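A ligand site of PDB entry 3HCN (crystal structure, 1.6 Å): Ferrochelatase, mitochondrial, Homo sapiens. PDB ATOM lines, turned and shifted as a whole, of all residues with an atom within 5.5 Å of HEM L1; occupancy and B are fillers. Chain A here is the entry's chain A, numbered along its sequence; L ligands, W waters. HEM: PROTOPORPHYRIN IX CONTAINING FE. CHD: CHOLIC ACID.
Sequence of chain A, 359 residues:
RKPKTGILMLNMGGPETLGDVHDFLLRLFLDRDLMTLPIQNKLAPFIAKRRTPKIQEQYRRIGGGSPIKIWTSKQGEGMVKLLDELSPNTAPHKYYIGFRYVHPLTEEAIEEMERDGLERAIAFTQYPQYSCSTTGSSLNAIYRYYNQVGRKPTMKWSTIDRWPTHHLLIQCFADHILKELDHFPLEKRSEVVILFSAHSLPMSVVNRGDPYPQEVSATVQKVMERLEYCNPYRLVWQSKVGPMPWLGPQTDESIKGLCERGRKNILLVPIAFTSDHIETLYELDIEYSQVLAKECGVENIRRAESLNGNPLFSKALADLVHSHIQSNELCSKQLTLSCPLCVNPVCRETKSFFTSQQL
O1D of HEM L1 sits at hydrogen-bond distance from N of Ile 278 (2.8 Å). An oxygen (O1A) of HEM L1 is in salt-bridge range of the guanidinium group (NE) of Arg 51, 2.4 Å away. A ring nitrogen (NE2) of His 199 sits at hydrogen-bond distance from an oxygen (O2D) of HEM L1. An oxygen (O26) of CHD L2 is in salt-bridge range of the guanidinium group (NH1) of Arg 51 (2.7 Å).
A ring nitrogen (NE2) of His 199 lies within hydrogen-bond range of the side-chain amide nitrogen (NE2) of Gln 238 (2.9 Å). O of His 199 lies within hydrogen-bond range of OH of Tyr 212, 2.7 Å away. The side-chain hydroxyl of Ser 131 sits at hydrogen-bond distance from the side-chain hydroxyl of Ser 133 (2.8 Å). O of Ser 131 lies within hydrogen-bond range of OG1 of Thr 134 (3.3 Å). N of Met 12 lies within hydrogen-bond range of OH of Tyr 127 (2.9 Å).
Met 12 touches HEM L1 (SD to C2D, 3.5 Å). CD2 of Leu 25 touches CAA of HEM L1, at 3.9 Å. Leu 28 touches HEM L1. Phe 29 touches HEM L1 (CZ to CMA, 3.5 Å). CD1 of Leu 34 touches C2B of HEM L1, at 3.7 Å. Ile 55 touches HEM L1. Tyr 59 touches HEM L1. Tyr 127 touches HEM L1 (CD2 to CBC, 3.7 Å). Ser 133 touches HEM L1. CG2 of Thr 134 touches C2C of HEM L1, 3.7 Å away. Leu 201 touches HEM L1 (CD2 to CAB, 3.7 Å). Pro 202 touches HEM L1 (CD to CAB, 3.4 Å). Val 205 touches HEM L1 (CG2 to CBB, 3.9 Å). CZ of Tyr 212 touches CMC of HEM L1, 3.7 Å away. Trp 246 touches HEM L1. Ala 272 touches HEM L1. CZ of Phe 273 touches CMD of HEM L1, 3.8 Å away. His 277 touches HEM L1 (CB to O1D, 3.0 Å). Of the 27 residues printed, 21 come within 4 Å of HEM L1.
Water W2 lies within hydrogen-bond range of O2D of HEM L1 (2.6 Å), O of Ile 278 (2.6 Å), NE2 of His 199 (3.0 Å) and NE2 of Gln 238 (3.0 Å). Water W1 lies within hydrogen-bond range of the side-chain hydroxyl of Tyr 59 (2.6 Å) and an oxygen (O1D) of HEM L1 (3.0 Å).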
ATOM      1  N   MET A  12      16.910  16.194  11.411  1.00  0.00           N
ATOM      2  CA  MET A  12      18.349  16.395  11.389  1.00  0.00           C
ATOM      3  C   MET A  12      18.748  17.586  10.524  1.00  0.00           C
ATOM      4  O   MET A  12      19.775  18.224  10.764  1.00  0.00           O
ATOM      5  CB  MET A  12      19.050  15.143  10.864  1.00  0.00           C
ATOM      6  CG  MET A  12      18.755  14.836   9.401  1.00  0.00           C
ATOM      7  SD  MET A  12      19.582  13.342   8.817  1.00  0.00           S
ATOM      8  CE  MET A  12      21.289  13.756   9.053  1.00  0.00           C
ATOM      9  N   PHE A  24      27.572  21.039   8.513  1.00  0.00           N
ATOM     10  CA  PHE A  24      26.560  20.002   8.707  1.00  0.00           C
ATOM     11  C   PHE A  24      27.250  18.790   9.316  1.00  0.00           C
ATOM     12  O   PHE A  24      26.802  18.252  10.343  1.00  0.00           O
ATOM     13  CB  PHE A  24      25.922  19.638   7.361  1.00  0.00           C
ATOM     14  CG  PHE A  24      25.114  18.364   7.380  1.00  0.00           C
ATOM     15  CD1 PHE A  24      23.939  18.265   8.119  1.00  0.00           C
ATOM     16  CD2 PHE A  24      25.520  17.273   6.616  1.00  0.00           C
ATOM     17  CE1 PHE A  24      23.183  17.091   8.107  1.00  0.00           C
ATOM     18  CE2 PHE A  24      24.772  16.088   6.592  1.00  0.00           C
ATOM     19  CZ  PHE A  24      23.601  16.009   7.334  1.00  0.00           C
ATOM     20  N   LEU A  25      28.345  18.368   8.690  1.00  0.00           N
ATOM     21  CA  LEU A  25      29.103  17.209   9.160  1.00  0.00           C
ATOM     22  C   LEU A  25      29.773  17.475  10.503  1.00  0.00           C
ATOM     23  O   LEU A  25      29.874  16.584  11.342  1.00  0.00           O
ATOM     24  CB  LEU A  25      30.151  16.817   8.120  1.00  0.00           C
ATOM     25  CG  LEU A  25      29.622  16.285   6.786  1.00  0.00           C
ATOM     26  CD1 LEU A  25      30.790  15.908   5.879  1.00  0.00           C
ATOM     27  CD2 LEU A  25      28.725  15.073   7.021  1.00  0.00           C
ATOM     28  N   LEU A  28      27.294  17.087  13.148  1.00  0.00           N
ATOM     29  CA  LEU A  28      26.868  15.685  13.185  1.00  0.00           C
ATOM     30  C   LEU A  28      27.877  14.821  13.935  1.00  0.00           C
ATOM     31  O   LEU A  28      27.502  14.063  14.841  1.00  0.00           O
ATOM     32  CB  LEU A  28      26.661  15.159  11.755  1.00  0.00           C
ATOM     33  CG  LEU A  28      26.050  13.763  11.606  1.00  0.00           C
ATOM     34  CD1 LEU A  28      25.281  13.667  10.294  1.00  0.00           C
ATOM     35  CD2 LEU A  28      27.141  12.704  11.670  1.00  0.00           C
ATOM     36  N   PHE A  29      29.160  14.933  13.592  1.00  0.00           N
ATOM     37  CA  PHE A  29      30.163  14.124  14.269  1.00  0.00           C
ATOM     38  C   PHE A  29      30.447  14.572  15.703  1.00  0.00           C
ATOM     39  O   PHE A  29      31.095  13.848  16.468  1.00  0.00           O
ATOM     40  CB  PHE A  29      31.455  14.079  13.455  1.00  0.00           C
ATOM     41  CG  PHE A  29      31.360  13.194  12.239  1.00  0.00           C
ATOM     42  CD1 PHE A  29      31.118  13.751  10.980  1.00  0.00           C
ATOM     43  CD2 PHE A  29      31.475  11.809  12.350  1.00  0.00           C
ATOM     44  CE1 PHE A  29      30.991  12.930   9.853  1.00  0.00           C
ATOM     45  CE2 PHE A  29      31.348  10.986  11.233  1.00  0.00           C
ATOM     46  CZ  PHE A  29      31.105  11.541   9.984  1.00  0.00           C
ATOM     47  N   LEU A  34      24.383  10.821  19.082  1.00  0.00           N
ATOM     48  CA  LEU A  34      24.403  10.051  17.853  1.00  0.00           C
ATOM     49  C   LEU A  34      25.483   8.978  17.893  1.00  0.00           C
ATOM     50  O   LEU A  34      25.227   7.808  17.655  1.00  0.00           O
ATOM     51  CB  LEU A  34      24.649  10.968  16.657  1.00  0.00           C
ATOM     52  CG  LEU A  34      24.882  10.268  15.323  1.00  0.00           C
ATOM     53  CD1 LEU A  34      23.664   9.416  14.983  1.00  0.00           C
ATOM     54  CD2 LEU A  34      25.138  11.309  14.230  1.00  0.00           C
ATOM     55  N   MET A  35      26.707   9.399  18.206  1.00  0.00           N
ATOM     56  CA  MET A  35      27.827   8.480  18.264  1.00  0.00           C
ATOM     57  C   MET A  35      28.801   8.886  19.357  1.00  0.00           C
ATOM     58  O   MET A  35      28.854  10.048  19.741  1.00  0.00           O
ATOM     59  CB  MET A  35      28.551   8.443  16.911  1.00  0.00           C
ATOM     60  CG  MET A  35      29.144   9.784  16.511  1.00  0.00           C
ATOM     61  SD  MET A  35      29.979   9.736  14.921  1.00  0.00           S
ATOM     62  CE  MET A  35      28.592  10.013  13.805  1.00  0.00           C
ATOM     63  N   ARG A  51      35.897  14.488   5.344  1.00  0.00           N
ATOM     64  CA  ARG A  51      34.768  13.814   4.714  1.00  0.00           C
ATOM     65  C   ARG A  51      33.887  14.733   3.861  1.00  0.00           C
ATOM     66  O   ARG A  51      33.038  14.256   3.101  1.00  0.00           O
ATOM     67  CB  ARG A  51      33.932  13.136   5.791  1.00  0.00           C
ATOM     68  CG  ARG A  51      33.149  11.930   5.335  1.00  0.00           C
ATOM     69  CD  ARG A  51      32.765  11.090   6.543  1.00  0.00           C
ATOM     70  NE  ARG A  51      31.929   9.950   6.185  1.00  0.00           N
ATOM     71  CZ  ARG A  51      32.294   8.956   5.382  1.00  0.00           C
ATOM     72  NH1 ARG A  51      33.511   8.950   4.843  1.00  0.00           N
ATOM     73  NH2 ARG A  51      31.447   7.980   5.100  1.00  0.00           N
ATOM     74  N   ILE A  55      31.002  13.861   0.640  1.00  0.00           N
ATOM     75  CA  ILE A  55      29.598  14.180   0.839  1.00  0.00           C
ATOM     76  C   ILE A  55      29.105  15.287  -0.097  1.00  0.00           C
ATOM     77  O   ILE A  55      27.954  15.257  -0.543  1.00  0.00           O
ATOM     78  CB  ILE A  55      29.330  14.584   2.306  1.00  0.00           C
ATOM     79  CG1 ILE A  55      29.821  13.468   3.240  1.00  0.00           C
ATOM     80  CG2 ILE A  55      27.855  14.862   2.524  1.00  0.00           C
ATOM     81  CD1 ILE A  55      29.293  12.082   2.886  1.00  0.00           C
ATOM     82  N   TYR A  59      25.926  15.025  -2.643  1.00  0.00           N
ATOM     83  CA  TYR A  59      24.813  15.965  -2.768  1.00  0.00           C
ATOM     84  C   TYR A  59      24.750  16.572  -4.158  1.00  0.00           C
ATOM     85  O   TYR A  59      23.677  16.925  -4.639  1.00  0.00           O
ATOM     86  CB  TYR A  59      24.906  17.062  -1.701  1.00  0.00           C
ATOM     87  CG  TYR A  59      24.314  16.635  -0.383  1.00  0.00           C
ATOM     88  CD1 TYR A  59      25.118  16.348   0.719  1.00  0.00           C
ATOM     89  CD2 TYR A  59      22.929  16.476  -0.248  1.00  0.00           C
ATOM     90  CE1 TYR A  59      24.560  15.914   1.927  1.00  0.00           C
ATOM     91  CE2 TYR A  59      22.362  16.045   0.950  1.00  0.00           C
ATOM     92  CZ  TYR A  59      23.189  15.767   2.034  1.00  0.00           C
ATOM     93  OH  TYR A  59      22.632  15.336   3.223  1.00  0.00           O
ATOM     94  N   TYR A 127      10.515  12.312  12.367  1.00  0.00           N
ATOM     95  CA  TYR A 127      10.905  10.936  12.063  1.00  0.00           C
ATOM     96  C   TYR A 127       9.727  10.111  12.583  1.00  0.00           C
ATOM     97  O   TYR A 127       9.466  10.085  13.788  1.00  0.00           O
ATOM     98  CB  TYR A 127      12.163  10.505  12.840  1.00  0.00           C
ATOM     99  CG  TYR A 127      13.419  11.322  12.629  1.00  0.00           C
ATOM    100  CD1 TYR A 127      13.729  12.386  13.474  1.00  0.00           C
ATOM    101  CD2 TYR A 127      14.323  10.982  11.627  1.00  0.00           C
ATOM    102  CE1 TYR A 127      14.937  13.086  13.332  1.00  0.00           C
ATOM    103  CE2 TYR A 127      15.530  11.675  11.474  1.00  0.00           C
ATOM    104  CZ  TYR A 127      15.827  12.728  12.336  1.00  0.00           C
ATOM    105  OH  TYR A 127      17.018  13.396  12.218  1.00  0.00           O
ATOM    106  N   SER A 131      14.256   6.454  16.957  1.00  0.00           N
ATOM    107  CA  SER A 131      15.599   5.912  17.154  1.00  0.00           C
ATOM    108  C   SER A 131      16.250   6.876  18.130  1.00  0.00           C
ATOM    109  O   SER A 131      16.006   8.082  18.062  1.00  0.00           O
ATOM    110  CB  SER A 131      16.426   5.894  15.873  1.00  0.00           C
ATOM    111  OG  SER A 131      17.735   5.412  16.178  1.00  0.00           O
ATOM    112  N   SER A 133      19.100   7.675  18.036  1.00  0.00           N
ATOM    113  CA  SER A 133      20.041   8.416  17.190  1.00  0.00           C
ATOM    114  C   SER A 133      19.421   9.596  16.450  1.00  0.00           C
ATOM    115  O   SER A 133      20.115  10.519  16.021  1.00  0.00           O
ATOM    116  CB  SER A 133      20.671   7.472  16.162  1.00  0.00           C
ATOM    117  OG  SER A 133      19.738   7.039  15.179  1.00  0.00           O
ATOM    118  N   THR A 134      18.106   9.569  16.285  1.00  0.00           N
ATOM    119  CA  THR A 134      17.422  10.634  15.562  1.00  0.00           C
ATOM    120  C   THR A 134      16.541  11.434  16.508  1.00  0.00           C
ATOM    121  O   THR A 134      16.960  12.462  17.020  1.00  0.00           O
ATOM    122  CB  THR A 134      16.606  10.035  14.399  1.00  0.00           C
ATOM    123  OG1 THR A 134      15.772   8.983  14.888  1.00  0.00           O
ATOM    124  CG2 THR A 134      17.538   9.463  13.331  1.00  0.00           C
ATOM    125  N   HIS A 199      17.189   3.727   6.522  1.00  0.00           N
ATOM    126  CA  HIS A 199      18.589   3.861   6.873  1.00  0.00           C
ATOM    127  C   HIS A 199      18.912   2.853   7.964  1.00  0.00           C
ATOM    128  O   HIS A 199      18.139   2.662   8.901  1.00  0.00           O
ATOM    129  CB  HIS A 199      18.911   5.269   7.387  1.00  0.00           C
ATOM    130  CG  HIS A 199      18.969   6.294   6.307  1.00  0.00           C
ATOM    131  ND1 HIS A 199      17.837   6.895   5.780  1.00  0.00           N
ATOM    132  CD2 HIS A 199      20.023   6.819   5.628  1.00  0.00           C
ATOM    133  CE1 HIS A 199      18.190   7.738   4.825  1.00  0.00           C
ATOM    134  NE2 HIS A 199      19.506   7.710   4.717  1.00  0.00           N
ATOM    135  N   SER A 200      20.062   2.198   7.833  1.00  0.00           N
ATOM    136  CA  SER A 200      20.483   1.195   8.790  1.00  0.00           C
ATOM    137  C   SER A 200      20.997   1.797  10.094  1.00  0.00           C
ATOM    138  O   SER A 200      21.154   3.014  10.230  1.00  0.00           O
ATOM    139  CB  SER A 200      21.581   0.327   8.165  1.00  0.00           C
ATOM    140  OG  SER A 200      21.944  -0.731   9.027  1.00  0.00           O
ATOM    141  N   LEU A 201      21.226   0.911  11.065  1.00  0.00           N
ATOM    142  CA  LEU A 201      21.765   1.280  12.374  1.00  0.00           C
ATOM    143  C   LEU A 201      22.955   0.350  12.649  1.00  0.00           C
ATOM    144  O   LEU A 201      22.982  -0.783  12.185  1.00  0.00           O
ATOM    145  CB  LEU A 201      20.752   1.052  13.490  1.00  0.00           C
ATOM    146  CG  LEU A 201      19.519   1.945  13.592  1.00  0.00           C
ATOM    147  CD1 LEU A 201      18.687   1.520  14.811  1.00  0.00           C
ATOM    148  CD2 LEU A 201      19.937   3.399  13.735  1.00  0.00           C
ATOM    149  N   PRO A 202      23.949   0.834  13.391  1.00  0.00           N
ATOM    150  CA  PRO A 202      25.085  -0.056  13.679  1.00  0.00           C
ATOM    151  C   PRO A 202      24.527  -1.169  14.575  1.00  0.00           C
ATOM    152  O   PRO A 202      23.624  -0.919  15.380  1.00  0.00           O
ATOM    153  CB  PRO A 202      26.041   0.853  14.455  1.00  0.00           C
ATOM    154  CG  PRO A 202      25.755   2.213  13.911  1.00  0.00           C
ATOM    155  CD  PRO A 202      24.237   2.211  13.827  1.00  0.00           C
ATOM    156  N   VAL A 205      24.130  -0.495  18.178  1.00  0.00           N
ATOM    157  CA  VAL A 205      22.989   0.317  18.578  1.00  0.00           C
ATOM    158  C   VAL A 205      21.748  -0.574  18.605  1.00  0.00           C
ATOM    159  O   VAL A 205      20.931  -0.483  19.513  1.00  0.00           O
ATOM    160  CB  VAL A 205      22.799   1.504  17.617  1.00  0.00           C
ATOM    161  CG1 VAL A 205      21.514   2.241  17.954  1.00  0.00           C
ATOM    162  CG2 VAL A 205      23.988   2.471  17.750  1.00  0.00           C
ATOM    163  N   TYR A 212      13.919   1.609  16.904  1.00  0.00           N
ATOM    164  CA  TYR A 212      13.751   1.840  15.477  1.00  0.00           C
ATOM    165  C   TYR A 212      13.422   0.662  14.541  1.00  0.00           C
ATOM    166  O   TYR A 212      12.430   0.702  13.813  1.00  0.00           O
ATOM    167  CB  TYR A 212      14.995   2.594  14.991  1.00  0.00           C
ATOM    168  CG  TYR A 212      15.101   2.907  13.505  1.00  0.00           C
ATOM    169  CD1 TYR A 212      14.450   4.020  12.944  1.00  0.00           C
ATOM    170  CD2 TYR A 212      15.948   2.173  12.689  1.00  0.00           C
ATOM    171  CE1 TYR A 212      14.660   4.371  11.595  1.00  0.00           C
ATOM    172  CE2 TYR A 212      16.164   2.508  11.368  1.00  0.00           C
ATOM    173  CZ  TYR A 212      15.532   3.615  10.818  1.00  0.00           C
ATOM    174  OH  TYR A 212      15.813   3.973   9.526  1.00  0.00           O
ATOM    175  N   GLN A 238      19.777   0.673   4.235  1.00  0.00           N
ATOM    176  CA  GLN A 238      20.871   1.339   3.531  1.00  0.00           C
ATOM    177  C   GLN A 238      21.921   1.805   4.548  1.00  0.00           C
ATOM    178  O   GLN A 238      21.643   2.639   5.403  1.00  0.00           O
ATOM    179  CB  GLN A 238      20.327   2.532   2.748  1.00  0.00           C
ATOM    180  CG  GLN A 238      19.545   3.541   3.572  1.00  0.00           C
ATOM    181  CD  GLN A 238      18.645   4.421   2.732  1.00  0.00           C
ATOM    182  OE1 GLN A 238      17.686   3.939   2.115  1.00  0.00           O
ATOM    183  NE2 GLN A 238      18.957   5.712   2.688  1.00  0.00           N
ATOM    184  N   VAL A 241      28.731   2.700   5.144  1.00  0.00           N
ATOM    185  CA  VAL A 241      29.433   3.901   5.593  1.00  0.00           C
ATOM    186  C   VAL A 241      30.699   3.561   6.375  1.00  0.00           C
ATOM    187  O   VAL A 241      31.633   4.363   6.432  1.00  0.00           O
ATOM    188  CB  VAL A 241      28.522   4.792   6.470  1.00  0.00           C
ATOM    189  CG1 VAL A 241      27.401   5.383   5.627  1.00  0.00           C
ATOM    190  CG2 VAL A 241      27.950   3.968   7.615  1.00  0.00           C
ATOM    191  N   TRP A 246      26.538  -3.450  10.571  1.00  0.00           N
ATOM    192  CA  TRP A 246      25.332  -2.642  10.590  1.00  0.00           C
ATOM    193  C   TRP A 246      24.199  -3.620  10.287  1.00  0.00           C
ATOM    194  O   TRP A 246      24.436  -4.694   9.725  1.00  0.00           O
ATOM    195  CB  TRP A 246      25.363  -1.548   9.509  1.00  0.00           C
ATOM    196  CG  TRP A 246      26.220  -0.357   9.846  1.00  0.00           C
ATOM    197  CD1 TRP A 246      27.571  -0.351  10.030  1.00  0.00           C
ATOM    198  CD2 TRP A 246      25.789   0.994  10.041  1.00  0.00           C
ATOM    199  NE1 TRP A 246      28.006   0.908  10.326  1.00  0.00           N
ATOM    200  CE2 TRP A 246      26.931   1.764  10.342  1.00  0.00           C
ATOM    201  CE3 TRP A 246      24.542   1.637   9.990  1.00  0.00           C
ATOM    202  CZ2 TRP A 246      26.870   3.138  10.589  1.00  0.00           C
ATOM    203  CZ3 TRP A 246      24.481   3.011  10.236  1.00  0.00           C
ATOM    204  CH2 TRP A 246      25.645   3.736  10.532  1.00  0.00           C
ATOM    205  N   ALA A 272      11.451   5.375   5.929  1.00  0.00           N
ATOM    206  CA  ALA A 272      11.803   5.979   7.220  1.00  0.00           C
ATOM    207  C   ALA A 272      12.394   7.390   7.187  1.00  0.00           C
ATOM    208  O   ALA A 272      12.926   7.866   8.187  1.00  0.00           O
ATOM    209  CB  ALA A 272      12.746   5.043   7.984  1.00  0.00           C
ATOM    210  N   PHE A 273      12.320   8.050   6.038  1.00  0.00           N
ATOM    211  CA  PHE A 273      12.804   9.421   5.940  1.00  0.00           C
ATOM    212  C   PHE A 273      11.955  10.045   4.849  1.00  0.00           C
ATOM    213  O   PHE A 273      12.043   9.673   3.689  1.00  0.00           O
ATOM    214  CB  PHE A 273      14.283   9.490   5.565  1.00  0.00           C
ATOM    215  CG  PHE A 273      14.938  10.797   5.936  1.00  0.00           C
ATOM    216  CD1 PHE A 273      15.208  11.101   7.264  1.00  0.00           C
ATOM    217  CD2 PHE A 273      15.221  11.740   4.961  1.00  0.00           C
ATOM    218  CE1 PHE A 273      15.747  12.339   7.626  1.00  0.00           C
ATOM    219  CE2 PHE A 273      15.771  12.979   5.303  1.00  0.00           C
ATOM    220  CZ  PHE A 273      16.040  13.282   6.642  1.00  0.00           C
ATOM    221  N   HIS A 277      16.818  12.245  -0.149  1.00  0.00           N
ATOM    222  CA  HIS A 277      18.138  12.082   0.442  1.00  0.00           C
ATOM    223  C   HIS A 277      19.064  11.350  -0.530  1.00  0.00           C
ATOM    224  O   HIS A 277      18.690  11.075  -1.669  1.00  0.00           O
ATOM    225  CB  HIS A 277      18.028  11.312   1.772  1.00  0.00           C
ATOM    226  CG  HIS A 277      17.146  10.108   1.715  1.00  0.00           C
ATOM    227  ND1 HIS A 277      15.765  10.194   1.686  1.00  0.00           N
ATOM    228  CD2 HIS A 277      17.444   8.787   1.668  1.00  0.00           C
ATOM    229  CE1 HIS A 277      15.257   8.976   1.645  1.00  0.00           C
ATOM    230  NE2 HIS A 277      16.247   8.105   1.630  1.00  0.00           N
ATOM    231  N   ILE A 278      20.283  11.058  -0.090  1.00  0.00           N
ATOM    232  CA  ILE A 278      21.245  10.381  -0.939  1.00  0.00           C
ATOM    233  C   ILE A 278      20.757   8.990  -1.311  1.00  0.00           C
ATOM    234  O   ILE A 278      20.330   8.219  -0.451  1.00  0.00           O
ATOM    235  CB  ILE A 278      22.627  10.292  -0.250  1.00  0.00           C
ATOM    236  CG1 ILE A 278      23.145  11.714   0.028  1.00  0.00           C
ATOM    237  CG2 ILE A 278      23.602   9.523  -1.123  1.00  0.00           C
ATOM    238  CD1 ILE A 278      24.460  11.763   0.775  1.00  0.00           C
HETATM  239  CHA HEM L   1      23.937  10.958   7.299  1.00  0.00           C
HETATM  240  CHB HEM L   1      25.537   8.312  10.904  1.00  0.00           C
HETATM  241  CHC HEM L   1      21.119   6.655  11.900  1.00  0.00           C
HETATM  242  CHD HEM L   1      19.469   9.294   8.219  1.00  0.00           C
HETATM  243  C1A HEM L   1      24.813  10.382   8.207  1.00  0.00           C
HETATM  244  C2A HEM L   1      26.202  10.601   8.255  1.00  0.00           C
HETATM  245  C3A HEM L   1      26.638   9.840   9.283  1.00  0.00           C
HETATM  246  C4A HEM L   1      25.524   9.147   9.869  1.00  0.00           C
HETATM  247  CMA HEM L   1      28.077   9.696   9.815  1.00  0.00           C
HETATM  248  CAA HEM L   1      27.035  11.642   7.530  1.00  0.00           C
HETATM  249  CBA HEM L   1      27.329  11.130   6.119  1.00  0.00           C
HETATM  250  CGA HEM L   1      28.617  10.368   5.860  1.00  0.00           C
HETATM  251  O1A HEM L   1      29.675  10.772   6.401  1.00  0.00           O
HETATM  252  O2A HEM L   1      28.583   9.430   5.118  1.00  0.00           O
HETATM  253  C1B HEM L   1      24.501   7.607  11.525  1.00  0.00           C
HETATM  254  C2B HEM L   1      24.687   6.742  12.660  1.00  0.00           C
HETATM  255  C3B HEM L   1      23.351   6.255  12.958  1.00  0.00           C
HETATM  256  C4B HEM L   1      22.513   6.855  11.996  1.00  0.00           C
HETATM  257  CMB HEM L   1      25.989   6.455  13.331  1.00  0.00           C
HETATM  258  CAB HEM L   1      23.030   5.343  14.037  1.00  0.00           C
HETATM  259  CBB HEM L   1      23.375   5.500  15.296  1.00  0.00           C
HETATM  260  C1C HEM L   1      20.267   7.244  10.955  1.00  0.00           C
HETATM  261  C2C HEM L   1      18.828   6.981  10.916  1.00  0.00           C
HETATM  262  C3C HEM L   1      18.301   7.737   9.841  1.00  0.00           C
HETATM  263  C4C HEM L   1      19.517   8.436   9.283  1.00  0.00           C
HETATM  264  CMC HEM L   1      18.071   6.061  11.869  1.00  0.00           C
HETATM  265  CAC HEM L   1      17.007   7.812   9.420  1.00  0.00           C
HETATM  266  CBC HEM L   1      15.837   8.083   9.873  1.00  0.00           C
HETATM  267  C1D HEM L   1      20.540   9.982   7.648  1.00  0.00           C
HETATM  268  C2D HEM L   1      20.391  10.919   6.478  1.00  0.00           C
HETATM  269  C3D HEM L   1      21.669  11.385   6.242  1.00  0.00           C
HETATM  270  C4D HEM L   1      22.562  10.753   7.213  1.00  0.00           C
HETATM  271  CMD HEM L   1      19.065  11.234   5.789  1.00  0.00           C
HETATM  272  CAD HEM L   1      22.059  12.468   5.298  1.00  0.00           C
HETATM  273  CBD HEM L   1      22.701  11.896   4.076  1.00  0.00           C
HETATM  274  CGD HEM L   1      21.827  10.954   3.402  1.00  0.00           C
HETATM  275  O1D HEM L   1      20.882  11.379   2.668  1.00  0.00           O
HETATM  276  O2D HEM L   1      22.013   9.732   3.565  1.00  0.00           O
HETATM  277  NA  HEM L   1      24.396   9.482   9.199  1.00  0.00           N
HETATM  278  NB  HEM L   1      23.240   7.695  11.120  1.00  0.00           N
HETATM  279  NC  HEM L   1      20.618   8.116   9.954  1.00  0.00           N
HETATM  280  ND  HEM L   1      21.820   9.927   8.030  1.00  0.00           N
HETATM  281 FE   HEM L   1      22.514   8.780   9.564  1.00  0.00          FE
HETATM  282  C1  CHD L   2      29.131   2.090  15.313  1.00  0.00           C
HETATM  283  C2  CHD L   2      30.264   1.096  15.665  1.00  0.00           C
HETATM  284  C3  CHD L   2      30.625   1.282  17.155  1.00  0.00           C
HETATM  285  O3  CHD L   2      31.659   0.357  17.520  1.00  0.00           O
HETATM  286  C4  CHD L   2      31.118   2.723  17.413  1.00  0.00           C
HETATM  287  C5  CHD L   2      30.031   3.780  17.004  1.00  0.00           C
HETATM  288  C6  CHD L   2      30.519   5.247  17.236  1.00  0.00           C
HETATM  289  C7  CHD L   2      31.646   5.660  16.229  1.00  0.00           C
HETATM  290  O7  CHD L   2      32.860   4.947  16.480  1.00  0.00           O
HETATM  291  C8  CHD L   2      31.188   5.450  14.749  1.00  0.00           C
HETATM  292  C9  CHD L   2      30.765   3.952  14.507  1.00  0.00           C
HETATM  293  C10 CHD L   2      29.584   3.571  15.504  1.00  0.00           C
HETATM  294  C11 CHD L   2      30.334   3.772  13.003  1.00  0.00           C
HETATM  295  C12 CHD L   2      31.513   4.161  12.078  1.00  0.00           C
HETATM  296  O12 CHD L   2      32.663   3.328  12.315  1.00  0.00           O
HETATM  297  C13 CHD L   2      31.926   5.649  12.267  1.00  0.00           C
HETATM  298  C14 CHD L   2      32.348   5.832  13.770  1.00  0.00           C
HETATM  299  C15 CHD L   2      32.824   7.295  13.798  1.00  0.00           C
HETATM  300  C16 CHD L   2      33.739   7.310  12.528  1.00  0.00           C
HETATM  301  C17 CHD L   2      33.178   6.231  11.520  1.00  0.00           C
HETATM  302  C18 CHD L   2      30.660   6.552  11.992  1.00  0.00           C
HETATM  303  C19 CHD L   2      28.344   4.447  15.176  1.00  0.00           C
HETATM  304  C20 CHD L   2      32.932   6.888  10.105  1.00  0.00           C
HETATM  305  C21 CHD L   2      32.366   5.840   9.101  1.00  0.00           C
HETATM  306  C22 CHD L   2      34.293   7.401   9.568  1.00  0.00           C
HETATM  307  C23 CHD L   2      34.184   8.088   8.188  1.00  0.00           C
HETATM  308  O25 CHD L   2      36.538   8.415   8.387  1.00  0.00           O
HETATM  309  C24 CHD L   2      35.539   8.582   7.709  1.00  0.00           C
HETATM  310  O26 CHD L   2      35.644   9.205   6.517  1.00  0.00           O
HETATM  311  O   HOH W   1      20.240  14.340   2.933  1.00  0.00           O
HETATM  312  O   HOH W   2      20.885   7.916   2.081  1.00  0.00           O
HETATM  313  O   HOH W   3      24.417   8.512   4.159  1.00  0.00           O
HETATM  314  O   HOH W   4      26.703   9.206   3.163  1.00  0.00           O
